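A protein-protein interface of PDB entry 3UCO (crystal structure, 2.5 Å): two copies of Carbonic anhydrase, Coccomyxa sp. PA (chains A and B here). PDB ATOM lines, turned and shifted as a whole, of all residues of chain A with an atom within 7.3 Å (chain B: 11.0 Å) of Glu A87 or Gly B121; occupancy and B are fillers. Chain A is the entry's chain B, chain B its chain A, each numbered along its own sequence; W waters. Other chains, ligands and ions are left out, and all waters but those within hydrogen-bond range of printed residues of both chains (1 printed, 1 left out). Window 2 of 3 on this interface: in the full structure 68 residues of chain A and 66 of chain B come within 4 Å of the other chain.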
ATOM      1  N   LEU A  43       6.279   4.026  -3.260  1.00  0.00           N
ATOM      2  CA  LEU A  43       5.901   5.438  -3.110  1.00  0.00           C
ATOM      3  C   LEU A  43       6.550   6.189  -4.267  1.00  0.00           C
ATOM      4  O   LEU A  43       7.741   6.011  -4.552  1.00  0.00           O
ATOM      5  CB  LEU A  43       6.390   6.020  -1.771  1.00  0.00           C
ATOM      6  CG  LEU A  43       6.399   7.537  -1.606  1.00  0.00           C
ATOM      7  CD1 LEU A  43       5.018   8.092  -1.538  1.00  0.00           C
ATOM      8  CD2 LEU A  43       7.144   7.882  -0.359  1.00  0.00           C
ATOM      9  N   LEU A  80       5.155  18.797   6.348  1.00  0.00           N
ATOM     10  CA  LEU A  80       4.473  17.625   6.906  1.00  0.00           C
ATOM     11  C   LEU A  80       3.577  16.959   5.913  1.00  0.00           C
ATOM     12  O   LEU A  80       3.169  15.824   6.118  1.00  0.00           O
ATOM     13  CB  LEU A  80       3.628  17.946   8.136  1.00  0.00           C
ATOM     14  CG  LEU A  80       4.308  18.595   9.343  1.00  0.00           C
ATOM     15  CD1 LEU A  80       3.266  18.916  10.345  1.00  0.00           C
ATOM     16  CD2 LEU A  80       5.400  17.715   9.961  1.00  0.00           C
ATOM     17  N   CYS A  82       4.503  16.292   2.568  1.00  0.00           N
ATOM     18  CA  CYS A  82       5.355  15.288   2.000  1.00  0.00           C
ATOM     19  C   CYS A  82       5.866  14.231   3.044  1.00  0.00           C
ATOM     20  O   CYS A  82       5.839  13.059   2.759  1.00  0.00           O
ATOM     21  CB  CYS A  82       6.490  15.924   1.193  1.00  0.00           C
ATOM     22  SG  CYS A  82       7.514  14.632   0.426  1.00  0.00           S
ATOM     23  N   MET A  83       6.312  14.653   4.232  1.00  0.00           N
ATOM     24  CA  MET A  83       6.861  13.748   5.269  1.00  0.00           C
ATOM     25  C   MET A  83       5.804  12.731   5.769  1.00  0.00           C
ATOM     26  O   MET A  83       6.128  11.584   6.098  1.00  0.00           O
ATOM     27  CB  MET A  83       7.355  14.547   6.432  1.00  0.00           C
ATOM     28  CG  MET A  83       8.728  15.185   6.192  1.00  0.00           C
ATOM     29  SD  MET A  83      10.098  14.015   5.918  1.00  0.00           S
ATOM     30  CE  MET A  83      10.547  14.437   4.268  1.00  0.00           C
ATOM     31  N   SER A  84       4.548  13.141   5.819  1.00  0.00           N
ATOM     32  CA  SER A  84       3.601  12.206   6.187  1.00  0.00           C
ATOM     33  C   SER A  84       3.325  11.187   5.064  1.00  0.00           C
ATOM     34  O   SER A  84       2.890  10.090   5.339  1.00  0.00           O
ATOM     35  CB  SER A  84       2.362  12.880   6.767  1.00  0.00           C
ATOM     36  OG  SER A  84       1.598  13.492   5.747  1.00  0.00           O
ATOM     37  N   CYS A  85       3.621  11.492   3.803  1.00  0.00           N
ATOM     38  CA  CYS A  85       3.487  10.453   2.806  1.00  0.00           C
ATOM     39  C   CYS A  85       4.608   9.451   3.015  1.00  0.00           C
ATOM     40  O   CYS A  85       4.400   8.261   2.901  1.00  0.00           O
ATOM     41  CB  CYS A  85       3.542  11.015   1.395  1.00  0.00           C
ATOM     42  SG  CYS A  85       1.985  11.720   0.916  1.00  0.00           S
ATOM     43  N   LEU A  86       5.790   9.977   3.314  1.00  0.00           N
ATOM     44  CA  LEU A  86       6.955   9.192   3.587  1.00  0.00           C
ATOM     45  C   LEU A  86       6.808   8.294   4.850  1.00  0.00           C
ATOM     46  O   LEU A  86       6.972   7.091   4.772  1.00  0.00           O
ATOM     47  CB  LEU A  86       8.134  10.139   3.697  1.00  0.00           C
ATOM     48  CG  LEU A  86       9.505   9.627   3.337  1.00  0.00           C
ATOM     49  CD1 LEU A  86       9.520   8.836   2.063  1.00  0.00           C
ATOM     50  CD2 LEU A  86      10.441  10.793   3.227  1.00  0.00           C
ATOM     51  N   GLU A  87       6.457   8.855   5.989  1.00  0.00           N
ATOM     52  CA  GLU A  87       6.356   8.079   7.213  1.00  0.00           C
ATOM     53  C   GLU A  87       5.254   6.997   7.107  1.00  0.00           C
ATOM     54  O   GLU A  87       5.486   5.832   7.416  1.00  0.00           O
ATOM     55  CB  GLU A  87       6.130   8.998   8.443  1.00  0.00           C
ATOM     56  CG  GLU A  87       5.953   8.252   9.705  1.00  0.00           C
ATOM     57  CD  GLU A  87       5.299   9.068  10.762  1.00  0.00           C
ATOM     58  OE1 GLU A  87       6.053   9.533  11.622  1.00  0.00           O
ATOM     59  OE2 GLU A  87       4.047   9.259  10.760  1.00  0.00           O
ATOM     60  N   TYR A  88       4.062   7.354   6.657  1.00  0.00           N
ATOM     61  CA  TYR A  88       3.001   6.372   6.598  1.00  0.00           C
ATOM     62  C   TYR A  88       3.316   5.226   5.672  1.00  0.00           C
ATOM     63  O   TYR A  88       2.875   4.084   5.925  1.00  0.00           O
ATOM     64  CB  TYR A  88       1.722   7.010   6.123  1.00  0.00           C
ATOM     65  CG  TYR A  88       0.487   6.093   6.183  1.00  0.00           C
ATOM     66  CD1 TYR A  88      -0.080   5.709   7.427  1.00  0.00           C
ATOM     67  CD2 TYR A  88      -0.126   5.650   5.016  1.00  0.00           C
ATOM     68  CE1 TYR A  88      -1.218   4.916   7.500  1.00  0.00           C
ATOM     69  CE2 TYR A  88      -1.256   4.877   5.067  1.00  0.00           C
ATOM     70  CZ  TYR A  88      -1.810   4.499   6.301  1.00  0.00           C
ATOM     71  OH  TYR A  88      -2.950   3.706   6.318  1.00  0.00           O
ATOM     72  N   THR A  89       3.986   5.502   4.555  1.00  0.00           N
ATOM     73  CA  THR A  89       4.259   4.413   3.601  1.00  0.00           C
ATOM     74  C   THR A  89       5.412   3.533   4.067  1.00  0.00           C
ATOM     75  O   THR A  89       5.350   2.335   3.892  1.00  0.00           O
ATOM     76  CB  THR A  89       4.597   4.869   2.163  1.00  0.00           C
ATOM     77  OG1 THR A  89       5.759   5.730   2.197  1.00  0.00           O
ATOM     78  CG2 THR A  89       3.365   5.473   1.488  1.00  0.00           C
ATOM     79  N   VAL A  90       6.475   4.140   4.593  1.00  0.00           N
ATOM     80  CA  VAL A  90       7.620   3.398   5.051  1.00  0.00           C
ATOM     81  C   VAL A  90       7.292   2.680   6.360  1.00  0.00           C
ATOM     82  O   VAL A  90       7.540   1.479   6.465  1.00  0.00           O
ATOM     83  CB  VAL A  90       8.846   4.285   5.198  1.00  0.00           C
ATOM     84  CG1 VAL A  90      10.024   3.524   5.888  1.00  0.00           C
ATOM     85  CG2 VAL A  90       9.247   4.765   3.843  1.00  0.00           C
ATOM     86  N   ASP A  91       6.696   3.361   7.319  1.00  0.00           N
ATOM     87  CA  ASP A  91       6.455   2.751   8.611  1.00  0.00           C
ATOM     88  C   ASP A  91       5.215   1.897   8.715  1.00  0.00           C
ATOM     89  O   ASP A  91       5.254   0.890   9.361  1.00  0.00           O
ATOM     90  CB  ASP A  91       6.456   3.792   9.713  1.00  0.00           C
ATOM     91  CG  ASP A  91       7.817   4.270  10.045  1.00  0.00           C
ATOM     92  OD1 ASP A  91       8.773   3.820   9.451  1.00  0.00           O
ATOM     93  OD2 ASP A  91       7.950   5.117  10.907  1.00  0.00           O
ATOM     94  N   HIS A  92       4.112   2.288   8.110  1.00  0.00           N
ATOM     95  CA  HIS A  92       2.880   1.522   8.303  1.00  0.00           C
ATOM     96  C   HIS A  92       2.669   0.544   7.176  1.00  0.00           C
ATOM     97  O   HIS A  92       2.406  -0.589   7.466  1.00  0.00           O
ATOM     98  CB  HIS A  92       1.602   2.374   8.524  1.00  0.00           C
ATOM     99  CG  HIS A  92       1.659   3.263   9.734  1.00  0.00           C
ATOM    100  ND1 HIS A  92       0.838   3.096  10.837  1.00  0.00           N
ATOM    101  CD2 HIS A  92       2.448   4.343  10.016  1.00  0.00           C
ATOM    102  CE1 HIS A  92       1.134   4.009  11.748  1.00  0.00           C
ATOM    103  NE2 HIS A  92       2.111   4.778  11.279  1.00  0.00           N
ATOM    104  N   LEU A  93       2.775   0.966   5.909  1.00  0.00           N
ATOM    105  CA  LEU A  93       2.493   0.109   4.741  1.00  0.00           C
ATOM    106  C   LEU A  93       3.709  -0.713   4.336  1.00  0.00           C
ATOM    107  O   LEU A  93       3.612  -1.687   3.570  1.00  0.00           O
ATOM    108  CB  LEU A  93       2.008   0.924   3.518  1.00  0.00           C
ATOM    109  CG  LEU A  93       0.708   1.688   3.631  1.00  0.00           C
ATOM    110  CD1 LEU A  93       0.392   2.429   2.342  1.00  0.00           C
ATOM    111  CD2 LEU A  93      -0.456   0.837   4.111  1.00  0.00           C
ATOM    112  N   LYS A  94       4.872  -0.296   4.810  1.00  0.00           N
ATOM    113  CA  LYS A  94       6.121  -1.008   4.488  1.00  0.00           C
ATOM    114  C   LYS A  94       6.367  -1.168   2.989  1.00  0.00           C
ATOM    115  O   LYS A  94       6.669  -2.268   2.533  1.00  0.00           O
ATOM    116  CB  LYS A  94       6.185  -2.367   5.221  1.00  0.00           C
ATOM    117  CG  LYS A  94       6.665  -2.243   6.671  1.00  0.00           C
ATOM    118  CD  LYS A  94       6.292  -3.492   7.490  1.00  0.00           C
ATOM    119  CE  LYS A  94       5.176  -3.150   8.528  1.00  0.00           C
ATOM    120  NZ  LYS A  94       5.714  -2.084   9.454  1.00  0.00           N
ATOM    121  N   ILE A 170      12.966   9.537   8.375  1.00  0.00           N
ATOM    122  CA  ILE A 170      12.139   8.334   8.174  1.00  0.00           C
ATOM    123  C   ILE A 170      13.014   7.245   7.527  1.00  0.00           C
ATOM    124  O   ILE A 170      13.076   6.121   8.022  1.00  0.00           O
ATOM    125  CB  ILE A 170      10.961   8.603   7.221  1.00  0.00           C
ATOM    126  CG1 ILE A 170      10.093   9.818   7.652  1.00  0.00           C
ATOM    127  CG2 ILE A 170      10.191   7.330   6.934  1.00  0.00           C
ATOM    128  CD1 ILE A 170       9.638   9.807   9.041  1.00  0.00           C
ATOM    129  N   ARG A 177      17.183  -0.021  11.158  1.00  0.00           N
ATOM    130  CA  ARG A 177      16.656  -1.243  11.738  1.00  0.00           C
ATOM    131  C   ARG A 177      16.618  -2.389  10.683  1.00  0.00           C
ATOM    132  O   ARG A 177      15.785  -3.325  10.788  1.00  0.00           O
ATOM    133  CB  ARG A 177      15.259  -0.986  12.308  1.00  0.00           C
ATOM    134  CG  ARG A 177      14.202  -0.611  11.297  1.00  0.00           C
ATOM    135  CD  ARG A 177      12.892  -0.184  11.958  1.00  0.00           C
ATOM    136  NE  ARG A 177      11.861   0.150  10.942  1.00  0.00           N
ATOM    137  CZ  ARG A 177      11.390   1.382  10.705  1.00  0.00           C
ATOM    138  NH1 ARG A 177      11.855   2.410  11.397  1.00  0.00           N
ATOM    139  NH2 ARG A 177      10.448   1.594   9.787  1.00  0.00           N
ATOM    140  N   ALA B  48      -3.396  10.471  -1.258  1.00  0.00           N
ATOM    141  CA  ALA B  48      -2.156   9.798  -1.702  1.00  0.00           C
ATOM    142  C   ALA B  48      -2.338   8.278  -1.901  1.00  0.00           C
ATOM    143  O   ALA B  48      -1.468   7.643  -2.501  1.00  0.00           O
ATOM    144  CB  ALA B  48      -1.061  10.048  -0.763  1.00  0.00           C
ATOM    145  N   VAL B  71      -2.074  12.849   2.272  1.00  0.00           N
ATOM    146  CA  VAL B  71      -2.705  11.856   3.115  1.00  0.00           C
ATOM    147  C   VAL B  71      -4.044  12.413   3.608  1.00  0.00           C
ATOM    148  O   VAL B  71      -4.066  13.214   4.494  1.00  0.00           O
ATOM    149  CB  VAL B  71      -1.776  11.366   4.298  1.00  0.00           C
ATOM    150  CG1 VAL B  71      -2.563  10.553   5.340  1.00  0.00           C
ATOM    151  CG2 VAL B  71      -0.648  10.544   3.770  1.00  0.00           C
ATOM    152  N   ALA B 108      -6.449   7.570   6.472  1.00  0.00           N
ATOM    153  CA  ALA B 108      -6.319   8.787   7.188  1.00  0.00           C
ATOM    154  C   ALA B 108      -7.611   9.089   7.919  1.00  0.00           C
ATOM    155  O   ALA B 108      -7.586   9.596   9.007  1.00  0.00           O
ATOM    156  CB  ALA B 108      -5.952   9.933   6.208  1.00  0.00           C
ATOM    157  N   ALA B 111      -7.625   6.690  10.995  1.00  0.00           N
ATOM    158  CA  ALA B 111      -6.713   7.145  12.052  1.00  0.00           C
ATOM    159  C   ALA B 111      -7.260   8.332  12.823  1.00  0.00           C
ATOM    160  O   ALA B 111      -7.080   8.445  14.053  1.00  0.00           O
ATOM    161  CB  ALA B 111      -5.351   7.504  11.466  1.00  0.00           C
ATOM    162  N   TRP B 115      -6.871   7.084  16.469  1.00  0.00           N
ATOM    163  CA  TRP B 115      -5.595   7.281  17.132  1.00  0.00           C
ATOM    164  C   TRP B 115      -5.731   8.201  18.318  1.00  0.00           C
ATOM    165  O   TRP B 115      -6.577   9.071  18.364  1.00  0.00           O
ATOM    166  CB  TRP B 115      -4.512   7.827  16.191  1.00  0.00           C
ATOM    167  CG  TRP B 115      -4.064   6.880  15.162  1.00  0.00           C
ATOM    168  CD1 TRP B 115      -4.532   5.630  14.959  1.00  0.00           C
ATOM    169  CD2 TRP B 115      -3.089   7.125  14.128  1.00  0.00           C
ATOM    170  NE1 TRP B 115      -3.908   5.068  13.868  1.00  0.00           N
ATOM    171  CE2 TRP B 115      -3.005   5.945  13.351  1.00  0.00           C
ATOM    172  CE3 TRP B 115      -2.257   8.204  13.820  1.00  0.00           C
ATOM    173  CZ2 TRP B 115      -2.137   5.801  12.279  1.00  0.00           C
ATOM    174  CZ3 TRP B 115      -1.384   8.079  12.745  1.00  0.00           C
ATOM    175  CH2 TRP B 115      -1.326   6.873  11.977  1.00  0.00           C
ATOM    176  N   HIS B 116      -4.875   7.993  19.298  1.00  0.00           N
ATOM    177  CA  HIS B 116      -4.873   8.832  20.481  1.00  0.00           C
ATOM    178  C   HIS B 116      -3.887   9.940  20.115  1.00  0.00           C
ATOM    179  O   HIS B 116      -2.831   9.656  19.559  1.00  0.00           O
ATOM    180  CB  HIS B 116      -4.367   8.017  21.697  1.00  0.00           C
ATOM    181  CG  HIS B 116      -4.428   8.762  23.002  1.00  0.00           C
ATOM    182  ND1 HIS B 116      -3.613   9.836  23.284  1.00  0.00           N
ATOM    183  CD2 HIS B 116      -5.213   8.588  24.096  1.00  0.00           C
ATOM    184  CE1 HIS B 116      -3.904  10.298  24.491  1.00  0.00           C
ATOM    185  NE2 HIS B 116      -4.877   9.565  25.000  1.00  0.00           N
ATOM    186  N   PRO B 117      -4.199  11.183  20.448  1.00  0.00           N
ATOM    187  CA  PRO B 117      -3.315  12.305  20.124  1.00  0.00           C
ATOM    188  C   PRO B 117      -1.890  12.123  20.648  1.00  0.00           C
ATOM    189  O   PRO B 117      -0.970  12.841  20.168  1.00  0.00           O
ATOM    190  CB  PRO B 117      -3.957  13.469  20.846  1.00  0.00           C
ATOM    191  CG  PRO B 117      -5.384  13.125  20.978  1.00  0.00           C
ATOM    192  CD  PRO B 117      -5.440  11.613  21.100  1.00  0.00           C
ATOM    193  N   LYS B 118      -1.662  11.195  21.590  1.00  0.00           N
ATOM    194  CA  LYS B 118      -0.319  11.007  22.072  1.00  0.00           C
ATOM    195  C   LYS B 118       0.583  10.320  21.053  1.00  0.00           C
ATOM    196  O   LYS B 118       1.848  10.389  21.165  1.00  0.00           O
ATOM    197  CB  LYS B 118      -0.288  10.250  23.414  1.00  0.00           C
ATOM    198  CG  LYS B 118      -0.465   8.678  23.407  1.00  0.00           C
ATOM    199  CD  LYS B 118      -0.923   8.284  24.810  1.00  0.00           C
ATOM    200  CE  LYS B 118      -1.249   6.768  24.984  1.00  0.00           C
ATOM    201  NZ  LYS B 118       0.048   6.048  24.971  1.00  0.00           N
ATOM    202  N   THR B 119      -0.029   9.673  20.060  1.00  0.00           N
ATOM    203  CA  THR B 119       0.698   8.817  19.139  1.00  0.00           C
ATOM    204  C   THR B 119       1.895   9.557  18.570  1.00  0.00           C
ATOM    205  O   THR B 119       1.770  10.692  18.128  1.00  0.00           O
ATOM    206  CB  THR B 119      -0.237   8.458  17.953  1.00  0.00           C
ATOM    207  OG1 THR B 119      -1.436   7.868  18.460  1.00  0.00           O
ATOM    208  CG2 THR B 119       0.410   7.456  17.021  1.00  0.00           C
ATOM    209  N   ALA B 120       3.060   8.933  18.550  1.00  0.00           N
ATOM    210  CA  ALA B 120       4.294   9.567  17.995  1.00  0.00           C
ATOM    211  C   ALA B 120       4.316   9.732  16.446  1.00  0.00           C
ATOM    212  O   ALA B 120       3.568   9.087  15.737  1.00  0.00           O
ATOM    213  CB  ALA B 120       5.496   8.734  18.417  1.00  0.00           C
ATOM    214  N   GLY B 121       5.221  10.559  15.940  1.00  0.00           N
ATOM    215  CA  GLY B 121       5.476  10.674  14.490  1.00  0.00           C
ATOM    216  C   GLY B 121       4.706  11.787  13.774  1.00  0.00           C
ATOM    217  O   GLY B 121       3.849  12.391  14.376  1.00  0.00           O
ATOM    218  N   VAL B 122       5.009  12.018  12.483  1.00  0.00           N
ATOM    219  CA  VAL B 122       4.413  13.103  11.671  1.00  0.00           C
ATOM    220  C   VAL B 122       3.029  12.835  11.112  1.00  0.00           C
ATOM    221  O   VAL B 122       2.224  13.772  11.019  1.00  0.00           O
ATOM    222  CB  VAL B 122       5.364  13.630  10.541  1.00  0.00           C
ATOM    223  CG1 VAL B 122       6.720  14.052  11.124  1.00  0.00           C
ATOM    224  CG2 VAL B 122       5.602  12.598   9.498  1.00  0.00           C
ATOM    225  N   THR B 123       2.682  11.595  10.772  1.00  0.00           N
ATOM    226  CA  THR B 123       1.271  11.364  10.287  1.00  0.00           C
ATOM    227  C   THR B 123       0.262  11.812  11.304  1.00  0.00           C
ATOM    228  O   THR B 123      -0.769  12.401  10.953  1.00  0.00           O
ATOM    229  CB  THR B 123       0.997   9.921   9.902  1.00  0.00           C
ATOM    230  OG1 THR B 123       1.987   9.514   8.970  1.00  0.00           O
ATOM    231  CG2 THR B 123      -0.395   9.727   9.226  1.00  0.00           C
ATOM    232  N   ASN B 124       0.555  11.571  12.580  1.00  0.00           N
ATOM    233  CA  ASN B 124      -0.347  12.006  13.663  1.00  0.00           C
ATOM    234  C   ASN B 124      -0.581  13.562  13.769  1.00  0.00           C
ATOM    235  O   ASN B 124      -1.698  14.046  14.088  1.00  0.00           O
ATOM    236  CB  ASN B 124       0.153  11.455  15.019  1.00  0.00           C
ATOM    237  CG  ASN B 124      -0.857  11.737  16.139  1.00  0.00           C
ATOM    238  OD1 ASN B 124      -2.052  11.424  16.007  1.00  0.00           O
ATOM    239  ND2 ASN B 124      -0.403  12.402  17.212  1.00  0.00           N
ATOM    240  N   LEU B 125       0.522  14.316  13.586  1.00  0.00           N
ATOM    241  CA  LEU B 125       0.489  15.773  13.466  1.00  0.00           C
ATOM    242  C   LEU B 125      -0.336  16.046  12.218  1.00  0.00           C
ATOM    243  O   LEU B 125      -1.345  16.741  12.277  1.00  0.00           O
ATOM    244  CB  LEU B 125       1.912  16.318  13.357  1.00  0.00           C
ATOM    245  CG  LEU B 125       2.843  16.029  14.582  1.00  0.00           C
ATOM    246  CD1 LEU B 125       4.187  16.668  14.398  1.00  0.00           C
ATOM    247  CD2 LEU B 125       2.222  16.548  15.923  1.00  0.00           C
ATOM    248  N   TRP B 126       0.014  15.406  11.115  1.00  0.00           N
ATOM    249  CA  TRP B 126      -0.603  15.745   9.859  1.00  0.00           C
ATOM    250  C   TRP B 126      -2.096  15.622   9.946  1.00  0.00           C
ATOM    251  O   TRP B 126      -2.804  16.534   9.508  1.00  0.00           O
ATOM    252  CB  TRP B 126      -0.031  14.936   8.697  1.00  0.00           C
ATOM    253  CG  TRP B 126      -0.741  15.153   7.423  1.00  0.00           C
ATOM    254  CD1 TRP B 126      -1.658  14.298   6.839  1.00  0.00           C
ATOM    255  CD2 TRP B 126      -0.691  16.319   6.563  1.00  0.00           C
ATOM    256  NE1 TRP B 126      -2.157  14.835   5.684  1.00  0.00           N
ATOM    257  CE2 TRP B 126      -1.585  16.073   5.481  1.00  0.00           C
ATOM    258  CE3 TRP B 126      -0.024  17.569   6.628  1.00  0.00           C
ATOM    259  CZ2 TRP B 126      -1.782  17.003   4.443  1.00  0.00           C
ATOM    260  CZ3 TRP B 126      -0.235  18.495   5.596  1.00  0.00           C
ATOM    261  CH2 TRP B 126      -1.103  18.210   4.534  1.00  0.00           C
ATOM    262  N   ILE B 127      -2.606  14.535  10.519  1.00  0.00           N
ATOM    263  CA  ILE B 127      -4.043  14.317  10.512  1.00  0.00           C
ATOM    264  C   ILE B 127      -4.836  15.065  11.556  1.00  0.00           C
ATOM    265  O   ILE B 127      -6.028  14.775  11.703  1.00  0.00           O
ATOM    266  CB  ILE B 127      -4.466  12.806  10.582  1.00  0.00           C
ATOM    267  CG1 ILE B 127      -3.965  12.149  11.892  1.00  0.00           C
ATOM    268  CG2 ILE B 127      -3.954  12.022   9.380  1.00  0.00           C
ATOM    269  CD1 ILE B 127      -4.892  11.231  12.452  1.00  0.00           C
ATOM    270  N   SER B 128      -4.257  16.047  12.253  1.00  0.00           N
ATOM    271  CA  SER B 128      -5.061  16.871  13.174  1.00  0.00           C
ATOM    272  C   SER B 128      -6.256  17.498  12.500  1.00  0.00           C
ATOM    273  O   SER B 128      -7.286  17.644  13.139  1.00  0.00           O
ATOM    274  CB  SER B 128      -4.231  17.975  13.816  1.00  0.00           C
ATOM    275  OG  SER B 128      -3.068  17.439  14.460  1.00  0.00           O
ATOM    276  N   ARG B 131      -9.260  15.105  12.925  1.00  0.00           N
ATOM    277  CA  ARG B 131      -9.806  15.247  14.287  1.00  0.00           C
ATOM    278  C   ARG B 131     -10.670  16.502  14.403  1.00  0.00           C
ATOM    279  O   ARG B 131     -11.767  16.450  14.916  1.00  0.00           O
ATOM    280  CB  ARG B 131      -8.737  15.220  15.354  1.00  0.00           C
ATOM    281  CG  ARG B 131      -8.119  13.807  15.512  1.00  0.00           C
ATOM    282  CD  ARG B 131      -7.197  13.734  16.690  1.00  0.00           C
ATOM    283  NE  ARG B 131      -5.922  14.410  16.434  1.00  0.00           N
ATOM    284  CZ  ARG B 131      -4.780  13.789  16.131  1.00  0.00           C
ATOM    285  NH1 ARG B 131      -4.688  12.437  16.065  1.00  0.00           N
ATOM    286  NH2 ARG B 131      -3.708  14.532  15.883  1.00  0.00           N
HETATM  287  O   HOH W   1       0.333  14.250   3.311  1.00  0.00           O
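The backbone NH (N) of Val B122 is in hydrogen-bond range of the side-chain carboxylate (OE1) of Glu A87.
The backbone NH (N) of Thr B123 sits at hydrogen-bond distance from the side-chain carboxylate (OE2) of Glu A87, at 2.7 Å.
The backbone carbonyl oxygen of Tyr A88 lies within hydrogen-bond range of the backbone NH of Leu A93 (3.1 Å).
O of Leu A80 lies within hydrogen-bond range of OG of Ser A84.
The indole nitrogen of Trp B126 is in hydrogen-bond range of the backbone carbonyl oxygen of Val B71.
O of Cys A85 sits at hydrogen-bond distance from OG1 of Thr A89 (3.0 Å).
Among the printed residues, merely in contact across the chains: Glu A87 with Gly B121, Ser A84 with Trp B126, Met A83 with Val B122, Leu A80 with Trp B126, His A92 with Trp B115, Tyr A88 with Thr B123, Ser A84 with Thr B123, Cys A85 with Ala B48, Ser A84 with Val B122 and Ser A84 with Val B71.
Ser A84 touches just these residues of chain B: Val B71 (3.9 Å), Val B122 (3.9 Å), Thr B123 (3.8 Å) and Trp B126 (3.3 Å).
Leu A86 touches none of the printed residues of chain B.
Of the printed residues of chain B, Glu A87 touches Gly B121 (3.1 Å), Val B122 (2.8 Å) and Thr B123 (2.7 Å).
Printed residues of chain B within 4 Å of His A92: Trp B115.
Printed residues of chain A within 4 Å of Val B71: Ser A84.
Gly B121 touches just one residue of chain A: Glu A87.
Printed residues of chain A within 4 Å of Thr B123: Ser A84, Glu A87 and Tyr A88.
The nearest residue of chain B that does not touch Glu A87 is Asn B124 (4.6 Å).
The nearest residue of chain A that does not touch Gly B121 is Ile A170 (6.9 Å).
Of the 17 printed residues of chain A, 7 touch a printed residue of chain B.
Hydrophobic or aromatic side chains of chain B within 4 Å of the printed part of chain A: Ala B48, Val B71, Trp B115, Val B122 and Trp B126.
No position is printed for both chains.
Of the 12 pairs that touch across the chains among the printed residues, none has its exchanged pair printed and touching as well.
Water W1 lies within hydrogen-bond range of the side-chain hydroxyl (OG) of Ser A84 (2.8 Å), the backbone NH (N) of Val B71 (3.0 Å) and the indole nitrogen (NE1) of Trp B126 (3.5 Å).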
